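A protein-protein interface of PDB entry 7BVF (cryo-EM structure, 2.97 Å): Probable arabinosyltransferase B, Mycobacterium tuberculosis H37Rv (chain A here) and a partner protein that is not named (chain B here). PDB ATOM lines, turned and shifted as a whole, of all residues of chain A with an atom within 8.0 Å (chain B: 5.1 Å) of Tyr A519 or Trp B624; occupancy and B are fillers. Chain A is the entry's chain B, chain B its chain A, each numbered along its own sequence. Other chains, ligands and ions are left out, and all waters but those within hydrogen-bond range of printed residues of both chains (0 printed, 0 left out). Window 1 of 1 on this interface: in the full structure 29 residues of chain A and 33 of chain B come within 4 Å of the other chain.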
ATOM      1  N   GLN A 516      18.203 -28.328 -17.852  1.00  0.00           N
ATOM      2  CA  GLN A 516      19.430 -27.807 -18.421  1.00  0.00           C
ATOM      3  C   GLN A 516      20.364 -28.941 -18.832  1.00  0.00           C
ATOM      4  O   GLN A 516      20.214 -30.091 -18.412  1.00  0.00           O
ATOM      5  CB  GLN A 516      20.130 -26.886 -17.424  1.00  0.00           C
ATOM      6  CG  GLN A 516      19.617 -25.460 -17.435  1.00  0.00           C
ATOM      7  CD  GLN A 516      18.643 -25.189 -16.312  1.00  0.00           C
ATOM      8  OE1 GLN A 516      18.349 -26.068 -15.506  1.00  0.00           O
ATOM      9  NE2 GLN A 516      18.136 -23.966 -16.253  1.00  0.00           N
ATOM     10  N   ALA A 517      21.337 -28.598 -19.669  1.00  0.00           N
ATOM     11  CA  ALA A 517      22.335 -29.547 -20.134  1.00  0.00           C
ATOM     12  C   ALA A 517      23.538 -29.550 -19.199  1.00  0.00           C
ATOM     13  O   ALA A 517      23.709 -28.666 -18.360  1.00  0.00           O
ATOM     14  CB  ALA A 517      22.760 -29.214 -21.560  1.00  0.00           C
ATOM     15  N   TRP A 518      24.385 -30.568 -19.351  1.00  0.00           N
ATOM     16  CA  TRP A 518      25.508 -30.735 -18.435  1.00  0.00           C
ATOM     17  C   TRP A 518      26.513 -29.596 -18.545  1.00  0.00           C
ATOM     18  O   TRP A 518      27.224 -29.307 -17.578  1.00  0.00           O
ATOM     19  CB  TRP A 518      26.198 -32.076 -18.679  1.00  0.00           C
ATOM     20  CG  TRP A 518      26.864 -32.184 -20.007  1.00  0.00           C
ATOM     21  CD1 TRP A 518      26.325 -32.682 -21.152  1.00  0.00           C
ATOM     22  CD2 TRP A 518      28.200 -31.789 -20.331  1.00  0.00           C
ATOM     23  NE1 TRP A 518      27.240 -32.618 -22.173  1.00  0.00           N
ATOM     24  CE2 TRP A 518      28.400 -32.073 -21.692  1.00  0.00           C
ATOM     25  CE3 TRP A 518      29.246 -31.218 -19.602  1.00  0.00           C
ATOM     26  CZ2 TRP A 518      29.599 -31.807 -22.338  1.00  0.00           C
ATOM     27  CZ3 TRP A 518      30.433 -30.954 -20.245  1.00  0.00           C
ATOM     28  CH2 TRP A 518      30.601 -31.248 -21.598  1.00  0.00           C
ATOM     29  N   TYR A 519      26.594 -28.939 -19.698  1.00  0.00           N
ATOM     30  CA  TYR A 519      27.564 -27.873 -19.896  1.00  0.00           C
ATOM     31  C   TYR A 519      27.066 -26.518 -19.418  1.00  0.00           C
ATOM     32  O   TYR A 519      27.775 -25.522 -19.580  1.00  0.00           O
ATOM     33  CB  TYR A 519      27.967 -27.784 -21.370  1.00  0.00           C
ATOM     34  CG  TYR A 519      26.818 -27.803 -22.344  1.00  0.00           C
ATOM     35  CD1 TYR A 519      26.087 -26.657 -22.605  1.00  0.00           C
ATOM     36  CD2 TYR A 519      26.473 -28.963 -23.015  1.00  0.00           C
ATOM     37  CE1 TYR A 519      25.043 -26.668 -23.496  1.00  0.00           C
ATOM     38  CE2 TYR A 519      25.431 -28.983 -23.907  1.00  0.00           C
ATOM     39  CZ  TYR A 519      24.718 -27.833 -24.144  1.00  0.00           C
ATOM     40  OH  TYR A 519      23.675 -27.846 -25.037  1.00  0.00           O
ATOM     41  N   THR A 520      25.871 -26.453 -18.836  1.00  0.00           N
ATOM     42  CA  THR A 520      25.359 -25.236 -18.213  1.00  0.00           C
ATOM     43  C   THR A 520      25.430 -25.322 -16.699  1.00  0.00           C
ATOM     44  O   THR A 520      24.560 -24.811 -15.994  1.00  0.00           O
ATOM     45  CB  THR A 520      23.930 -24.961 -18.662  1.00  0.00           C
ATOM     46  OG1 THR A 520      23.044 -25.844 -17.974  1.00  0.00           O
ATOM     47  CG2 THR A 520      23.789 -25.177 -20.152  1.00  0.00           C
ATOM     48  N   GLU A 521      26.467 -25.976 -16.177  1.00  0.00           N
ATOM     49  CA  GLU A 521      26.617 -26.134 -14.739  1.00  0.00           C
ATOM     50  C   GLU A 521      27.026 -24.838 -14.054  1.00  0.00           C
ATOM     51  O   GLU A 521      26.746 -24.666 -12.864  1.00  0.00           O
ATOM     52  CB  GLU A 521      27.631 -27.244 -14.455  1.00  0.00           C
ATOM     53  CG  GLU A 521      28.203 -27.275 -13.046  1.00  0.00           C
ATOM     54  CD  GLU A 521      27.242 -27.842 -12.017  1.00  0.00           C
ATOM     55  OE1 GLU A 521      26.069 -28.094 -12.359  1.00  0.00           O
ATOM     56  OE2 GLU A 521      27.665 -28.039 -10.858  1.00  0.00           O
ATOM     57  N   ASN A 522      27.647 -23.907 -14.780  1.00  0.00           N
ATOM     58  CA  ASN A 522      28.077 -22.652 -14.177  1.00  0.00           C
ATOM     59  C   ASN A 522      26.919 -21.798 -13.681  1.00  0.00           C
ATOM     60  O   ASN A 522      27.157 -20.835 -12.948  1.00  0.00           O
ATOM     61  CB  ASN A 522      28.919 -21.851 -15.171  1.00  0.00           C
ATOM     62  CG  ASN A 522      28.262 -21.723 -16.529  1.00  0.00           C
ATOM     63  OD1 ASN A 522      27.051 -21.551 -16.637  1.00  0.00           O
ATOM     64  ND2 ASN A 522      29.065 -21.804 -17.578  1.00  0.00           N
ATOM     65  N   LEU A 523      25.681 -22.120 -14.060  1.00  0.00           N
ATOM     66  CA  LEU A 523      24.536 -21.381 -13.543  1.00  0.00           C
ATOM     67  C   LEU A 523      24.386 -21.575 -12.043  1.00  0.00           C
ATOM     68  O   LEU A 523      23.986 -20.649 -11.327  1.00  0.00           O
ATOM     69  CB  LEU A 523      23.264 -21.817 -14.261  1.00  0.00           C
ATOM     70  CG  LEU A 523      23.053 -21.272 -15.668  1.00  0.00           C
ATOM     71  CD1 LEU A 523      21.809 -21.878 -16.275  1.00  0.00           C
ATOM     72  CD2 LEU A 523      22.947 -19.764 -15.628  1.00  0.00           C
ATOM     73  N   PHE A 583      31.281 -33.678  -9.158  1.00  0.00           N
ATOM     74  CA  PHE A 583      31.261 -34.088 -10.559  1.00  0.00           C
ATOM     75  C   PHE A 583      29.915 -34.688 -10.955  1.00  0.00           C
ATOM     76  O   PHE A 583      29.429 -34.443 -12.063  1.00  0.00           O
ATOM     77  CB  PHE A 583      32.390 -35.083 -10.828  1.00  0.00           C
ATOM     78  CG  PHE A 583      32.243 -35.838 -12.118  1.00  0.00           C
ATOM     79  CD1 PHE A 583      32.578 -35.248 -13.323  1.00  0.00           C
ATOM     80  CD2 PHE A 583      31.785 -37.144 -12.125  1.00  0.00           C
ATOM     81  CE1 PHE A 583      32.448 -35.942 -14.508  1.00  0.00           C
ATOM     82  CE2 PHE A 583      31.652 -37.841 -13.307  1.00  0.00           C
ATOM     83  CZ  PHE A 583      31.985 -37.240 -14.499  1.00  0.00           C
ATOM     84  N   MET A 586      26.772 -32.509 -11.781  1.00  0.00           N
ATOM     85  CA  MET A 586      26.746 -31.825 -13.064  1.00  0.00           C
ATOM     86  C   MET A 586      25.674 -32.382 -13.988  1.00  0.00           C
ATOM     87  O   MET A 586      25.131 -31.642 -14.813  1.00  0.00           O
ATOM     88  CB  MET A 586      28.118 -31.935 -13.723  1.00  0.00           C
ATOM     89  CG  MET A 586      28.394 -30.921 -14.798  1.00  0.00           C
ATOM     90  SD  MET A 586      30.131 -30.952 -15.267  1.00  0.00           S
ATOM     91  CE  MET A 586      30.318 -32.674 -15.713  1.00  0.00           C
ATOM     92  N   PHE A 587      25.364 -33.667 -13.873  1.00  0.00           N
ATOM     93  CA  PHE A 587      24.361 -34.324 -14.711  1.00  0.00           C
ATOM     94  C   PHE A 587      22.989 -34.332 -14.049  1.00  0.00           C
ATOM     95  O   PHE A 587      22.360 -35.378 -13.916  1.00  0.00           O
ATOM     96  CB  PHE A 587      24.806 -35.742 -15.037  1.00  0.00           C
ATOM     97  CG  PHE A 587      26.151 -35.816 -15.688  1.00  0.00           C
ATOM     98  CD1 PHE A 587      26.287 -35.607 -17.046  1.00  0.00           C
ATOM     99  CD2 PHE A 587      27.278 -36.096 -14.945  1.00  0.00           C
ATOM    100  CE1 PHE A 587      27.520 -35.674 -17.645  1.00  0.00           C
ATOM    101  CE2 PHE A 587      28.514 -36.162 -15.542  1.00  0.00           C
ATOM    102  CZ  PHE A 587      28.633 -35.951 -16.894  1.00  0.00           C
ATOM    103  N   LYS A 591      19.421 -26.857 -12.104  1.00  0.00           N
ATOM    104  CA  LYS A 591      20.592 -26.279 -11.457  1.00  0.00           C
ATOM    105  C   LYS A 591      20.113 -25.206 -10.486  1.00  0.00           C
ATOM    106  O   LYS A 591      20.074 -24.020 -10.809  1.00  0.00           O
ATOM    107  CB  LYS A 591      21.559 -25.702 -12.504  1.00  0.00           C
ATOM    108  CG  LYS A 591      21.813 -26.601 -13.703  1.00  0.00           C
ATOM    109  CD  LYS A 591      22.794 -27.701 -13.365  1.00  0.00           C
ATOM    110  CE  LYS A 591      23.287 -28.420 -14.601  1.00  0.00           C
ATOM    111  NZ  LYS A 591      22.239 -29.271 -15.204  1.00  0.00           N
ATOM    112  N   GLU B 516      25.789 -19.415 -22.817  1.00  0.00           N
ATOM    113  CA  GLU B 516      25.113 -20.231 -23.821  1.00  0.00           C
ATOM    114  C   GLU B 516      25.488 -19.938 -25.271  1.00  0.00           C
ATOM    115  O   GLU B 516      26.160 -20.761 -25.899  1.00  0.00           O
ATOM    116  CB  GLU B 516      23.600 -20.081 -23.659  1.00  0.00           C
ATOM    117  CG  GLU B 516      22.793 -21.185 -24.315  1.00  0.00           C
ATOM    118  CD  GLU B 516      22.788 -22.466 -23.506  1.00  0.00           C
ATOM    119  OE1 GLU B 516      23.244 -22.437 -22.345  1.00  0.00           O
ATOM    120  OE2 GLU B 516      22.328 -23.501 -24.031  1.00  0.00           O
ATOM    121  N   ARG B 526      36.903 -20.128 -25.294  1.00  0.00           N
ATOM    122  CA  ARG B 526      36.947 -21.022 -24.146  1.00  0.00           C
ATOM    123  C   ARG B 526      38.201 -21.879 -24.168  1.00  0.00           C
ATOM    124  O   ARG B 526      38.755 -22.199 -23.115  1.00  0.00           O
ATOM    125  CB  ARG B 526      35.716 -21.920 -24.122  1.00  0.00           C
ATOM    126  CG  ARG B 526      34.407 -21.211 -24.262  1.00  0.00           C
ATOM    127  CD  ARG B 526      33.285 -22.194 -24.073  1.00  0.00           C
ATOM    128  NE  ARG B 526      31.991 -21.599 -24.358  1.00  0.00           N
ATOM    129  CZ  ARG B 526      30.835 -22.155 -24.031  1.00  0.00           C
ATOM    130  NH1 ARG B 526      29.701 -21.543 -24.326  1.00  0.00           N
ATOM    131  NH2 ARG B 526      30.816 -23.321 -23.405  1.00  0.00           N
ATOM    132  N   LEU B 530      40.732 -22.404 -21.008  1.00  0.00           N
ATOM    133  CA  LEU B 530      40.741 -23.704 -20.350  1.00  0.00           C
ATOM    134  C   LEU B 530      42.106 -24.360 -20.463  1.00  0.00           C
ATOM    135  O   LEU B 530      42.570 -24.998 -19.514  1.00  0.00           O
ATOM    136  CB  LEU B 530      39.657 -24.600 -20.945  1.00  0.00           C
ATOM    137  CG  LEU B 530      38.219 -24.123 -20.736  1.00  0.00           C
ATOM    138  CD1 LEU B 530      37.245 -25.094 -21.365  1.00  0.00           C
ATOM    139  CD2 LEU B 530      37.921 -23.937 -19.265  1.00  0.00           C
ATOM    140  N   PHE B 620      38.213 -33.910 -22.047  1.00  0.00           N
ATOM    141  CA  PHE B 620      37.200 -33.190 -21.285  1.00  0.00           C
ATOM    142  C   PHE B 620      37.252 -31.692 -21.572  1.00  0.00           C
ATOM    143  O   PHE B 620      36.209 -31.033 -21.683  1.00  0.00           O
ATOM    144  CB  PHE B 620      37.398 -33.481 -19.801  1.00  0.00           C
ATOM    145  CG  PHE B 620      36.226 -33.129 -18.949  1.00  0.00           C
ATOM    146  CD1 PHE B 620      34.961 -33.581 -19.271  1.00  0.00           C
ATOM    147  CD2 PHE B 620      36.397 -32.395 -17.793  1.00  0.00           C
ATOM    148  CE1 PHE B 620      33.883 -33.268 -18.481  1.00  0.00           C
ATOM    149  CE2 PHE B 620      35.325 -32.087 -16.996  1.00  0.00           C
ATOM    150  CZ  PHE B 620      34.066 -32.524 -17.339  1.00  0.00           C
ATOM    151  N   VAL B 621      38.458 -31.139 -21.705  1.00  0.00           N
ATOM    152  CA  VAL B 621      38.589 -29.735 -22.091  1.00  0.00           C
ATOM    153  C   VAL B 621      38.000 -29.502 -23.478  1.00  0.00           C
ATOM    154  O   VAL B 621      37.328 -28.494 -23.720  1.00  0.00           O
ATOM    155  CB  VAL B 621      40.062 -29.297 -22.016  1.00  0.00           C
ATOM    156  CG1 VAL B 621      40.257 -27.969 -22.707  1.00  0.00           C
ATOM    157  CG2 VAL B 621      40.510 -29.208 -20.569  1.00  0.00           C
ATOM    158  N   LEU B 622      38.240 -30.427 -24.409  1.00  0.00           N
ATOM    159  CA  LEU B 622      37.649 -30.301 -25.741  1.00  0.00           C
ATOM    160  C   LEU B 622      36.128 -30.383 -25.685  1.00  0.00           C
ATOM    161  O   LEU B 622      35.431 -29.688 -26.438  1.00  0.00           O
ATOM    162  CB  LEU B 622      38.205 -31.379 -26.666  1.00  0.00           C
ATOM    163  CG  LEU B 622      39.420 -31.004 -27.510  1.00  0.00           C
ATOM    164  CD1 LEU B 622      39.996 -32.239 -28.167  1.00  0.00           C
ATOM    165  CD2 LEU B 622      39.043 -29.974 -28.552  1.00  0.00           C
ATOM    166  N   ALA B 623      35.595 -31.236 -24.809  1.00  0.00           N
ATOM    167  CA  ALA B 623      34.149 -31.332 -24.646  1.00  0.00           C
ATOM    168  C   ALA B 623      33.563 -30.027 -24.127  1.00  0.00           C
ATOM    169  O   ALA B 623      32.483 -29.610 -24.558  1.00  0.00           O
ATOM    170  CB  ALA B 623      33.804 -32.483 -23.705  1.00  0.00           C
ATOM    171  N   TRP B 624      34.251 -29.370 -23.191  1.00  0.00           N
ATOM    172  CA  TRP B 624      33.786 -28.059 -22.741  1.00  0.00           C
ATOM    173  C   TRP B 624      33.874 -27.028 -23.860  1.00  0.00           C
ATOM    174  O   TRP B 624      32.948 -26.237 -24.060  1.00  0.00           O
ATOM    175  CB  TRP B 624      34.581 -27.580 -21.526  1.00  0.00           C
ATOM    176  CG  TRP B 624      34.207 -28.223 -20.242  1.00  0.00           C
ATOM    177  CD1 TRP B 624      34.825 -29.278 -19.641  1.00  0.00           C
ATOM    178  CD2 TRP B 624      33.134 -27.841 -19.373  1.00  0.00           C
ATOM    179  NE1 TRP B 624      34.196 -29.587 -18.463  1.00  0.00           N
ATOM    180  CE2 TRP B 624      33.155 -28.720 -18.275  1.00  0.00           C
ATOM    181  CE3 TRP B 624      32.154 -26.846 -19.423  1.00  0.00           C
ATOM    182  CZ2 TRP B 624      32.235 -28.635 -17.234  1.00  0.00           C
ATOM    183  CZ3 TRP B 624      31.238 -26.762 -18.387  1.00  0.00           C
ATOM    184  CH2 TRP B 624      31.289 -27.652 -17.310  1.00  0.00           C
ATOM    185  N   ALA B 625      34.979 -27.029 -24.605  1.00  0.00           N
ATOM    186  CA  ALA B 625      35.198 -25.990 -25.607  1.00  0.00           C
ATOM    187  C   ALA B 625      34.175 -26.079 -26.728  1.00  0.00           C
ATOM    188  O   ALA B 625      33.533 -25.082 -27.074  1.00  0.00           O
ATOM    189  CB  ALA B 625      36.614 -26.091 -26.166  1.00  0.00           C
ATOM    190  N   THR B 626      33.992 -27.266 -27.304  1.00  0.00           N
ATOM    191  CA  THR B 626      33.096 -27.396 -28.454  1.00  0.00           C
ATOM    192  C   THR B 626      31.636 -27.491 -28.053  1.00  0.00           C
ATOM    193  O   THR B 626      30.912 -28.362 -28.534  1.00  0.00           O
ATOM    194  CB  THR B 626      33.499 -28.611 -29.283  1.00  0.00           C
ATOM    195  OG1 THR B 626      33.687 -29.736 -28.420  1.00  0.00           O
ATOM    196  CG2 THR B 626      34.784 -28.342 -30.033  1.00  0.00           C
ATOM    197  N   SER B 627      31.172 -26.578 -27.207  1.00  0.00           N
ATOM    198  CA  SER B 627      29.777 -26.512 -26.807  1.00  0.00           C
ATOM    199  C   SER B 627      29.214 -25.111 -26.942  1.00  0.00           C
ATOM    200  O   SER B 627      28.043 -24.893 -26.616  1.00  0.00           O
ATOM    201  CB  SER B 627      29.604 -27.000 -25.366  1.00  0.00           C
ATOM    202  OG  SER B 627      29.908 -25.973 -24.444  1.00  0.00           O
ATOM    203  N   GLY B 628      30.021 -24.152 -27.398  1.00  0.00           N
ATOM    204  CA  GLY B 628      29.556 -22.832 -27.742  1.00  0.00           C
ATOM    205  C   GLY B 628      29.641 -22.628 -29.244  1.00  0.00           C
ATOM    206  O   GLY B 628      30.287 -23.379 -29.968  1.00  0.00           O
ATOM    207  N   GLN B 646      25.883 -24.581 -32.194  1.00  0.00           N
ATOM    208  CA  GLN B 646      27.090 -25.272 -31.787  1.00  0.00           C
ATOM    209  C   GLN B 646      27.442 -26.352 -32.803  1.00  0.00           C
ATOM    210  O   GLN B 646      26.570 -26.851 -33.516  1.00  0.00           O
ATOM    211  CB  GLN B 646      26.915 -25.869 -30.396  1.00  0.00           C
ATOM    212  CG  GLN B 646      25.686 -26.715 -30.215  1.00  0.00           C
ATOM    213  CD  GLN B 646      25.562 -27.224 -28.798  1.00  0.00           C
ATOM    214  OE1 GLN B 646      26.163 -26.675 -27.879  1.00  0.00           O
ATOM    215  NE2 GLN B 646      24.787 -28.281 -28.615  1.00  0.00           N
ATOM    216  N   THR B 655      29.896 -32.018 -28.721  1.00  0.00           N
ATOM    217  CA  THR B 655      30.191 -31.912 -27.299  1.00  0.00           C
ATOM    218  C   THR B 655      29.794 -33.154 -26.514  1.00  0.00           C
ATOM    219  O   THR B 655      30.218 -33.296 -25.364  1.00  0.00           O
ATOM    220  CB  THR B 655      29.492 -30.686 -26.715  1.00  0.00           C
ATOM    221  OG1 THR B 655      29.908 -30.497 -25.359  1.00  0.00           O
ATOM    222  CG2 THR B 655      27.989 -30.857 -26.758  1.00  0.00           C
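The side-chain hydroxyl (OG1) of Thr A520 lies within hydrogen-bond range of the backbone carbonyl oxygen (O) of Ala A517, at 2.9 Å.
OG1 of Thr B655 is in hydrogen-bond range of O of Ala B623 (2.8 Å).
OG of Ser B627 is in hydrogen-bond range of O of Trp B624 (3.1 Å).
The side-chain amide oxygen (OE1) of Gln B646 lies close to the backbone carbonyl oxygen (O) of Ser B627, 2.9 Å away.
Hydrophobic or aromatic side chains of chain A within 4 Å of the printed part of chain B: Trp A518, Tyr A519 and Met A586.
Among the printed residues, 6 pairs touch across the chains.
Trp B624 touches two residues of chain A.
No residue of chain A comes within 4 Å of Ala B625.
Of the printed residues of chain A, Glu B516 touches Thr A520 (3.6 Å).
Of the printed residues of chain B, Trp A518 touches Ala B623 and Thr B655.
Of the printed residues of chain A, Thr B655 touches Trp A518.
Gly B628 touches none of the printed residues of chain A.
Phe A587 touches none of the printed residues of chain B.
The nearest residue of chain B that does not touch Tyr A519 is Ser B627 (4.1 Å).
The nearest residue of chain A that does not touch Trp B624 is Trp A518 (4.03 Å).
The nearest printed residue of chain B that does not touch Met A586 is Phe B620 (4.1 Å).
Among the printed residues, pairs that only touch across the chains: Trp A518 with Ala B623, Trp A518 with Thr B655, Tyr A519 with Trp B624, Tyr A519 with Gln B646, Thr A520 with Glu B516 and Met A586 with Trp B624.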
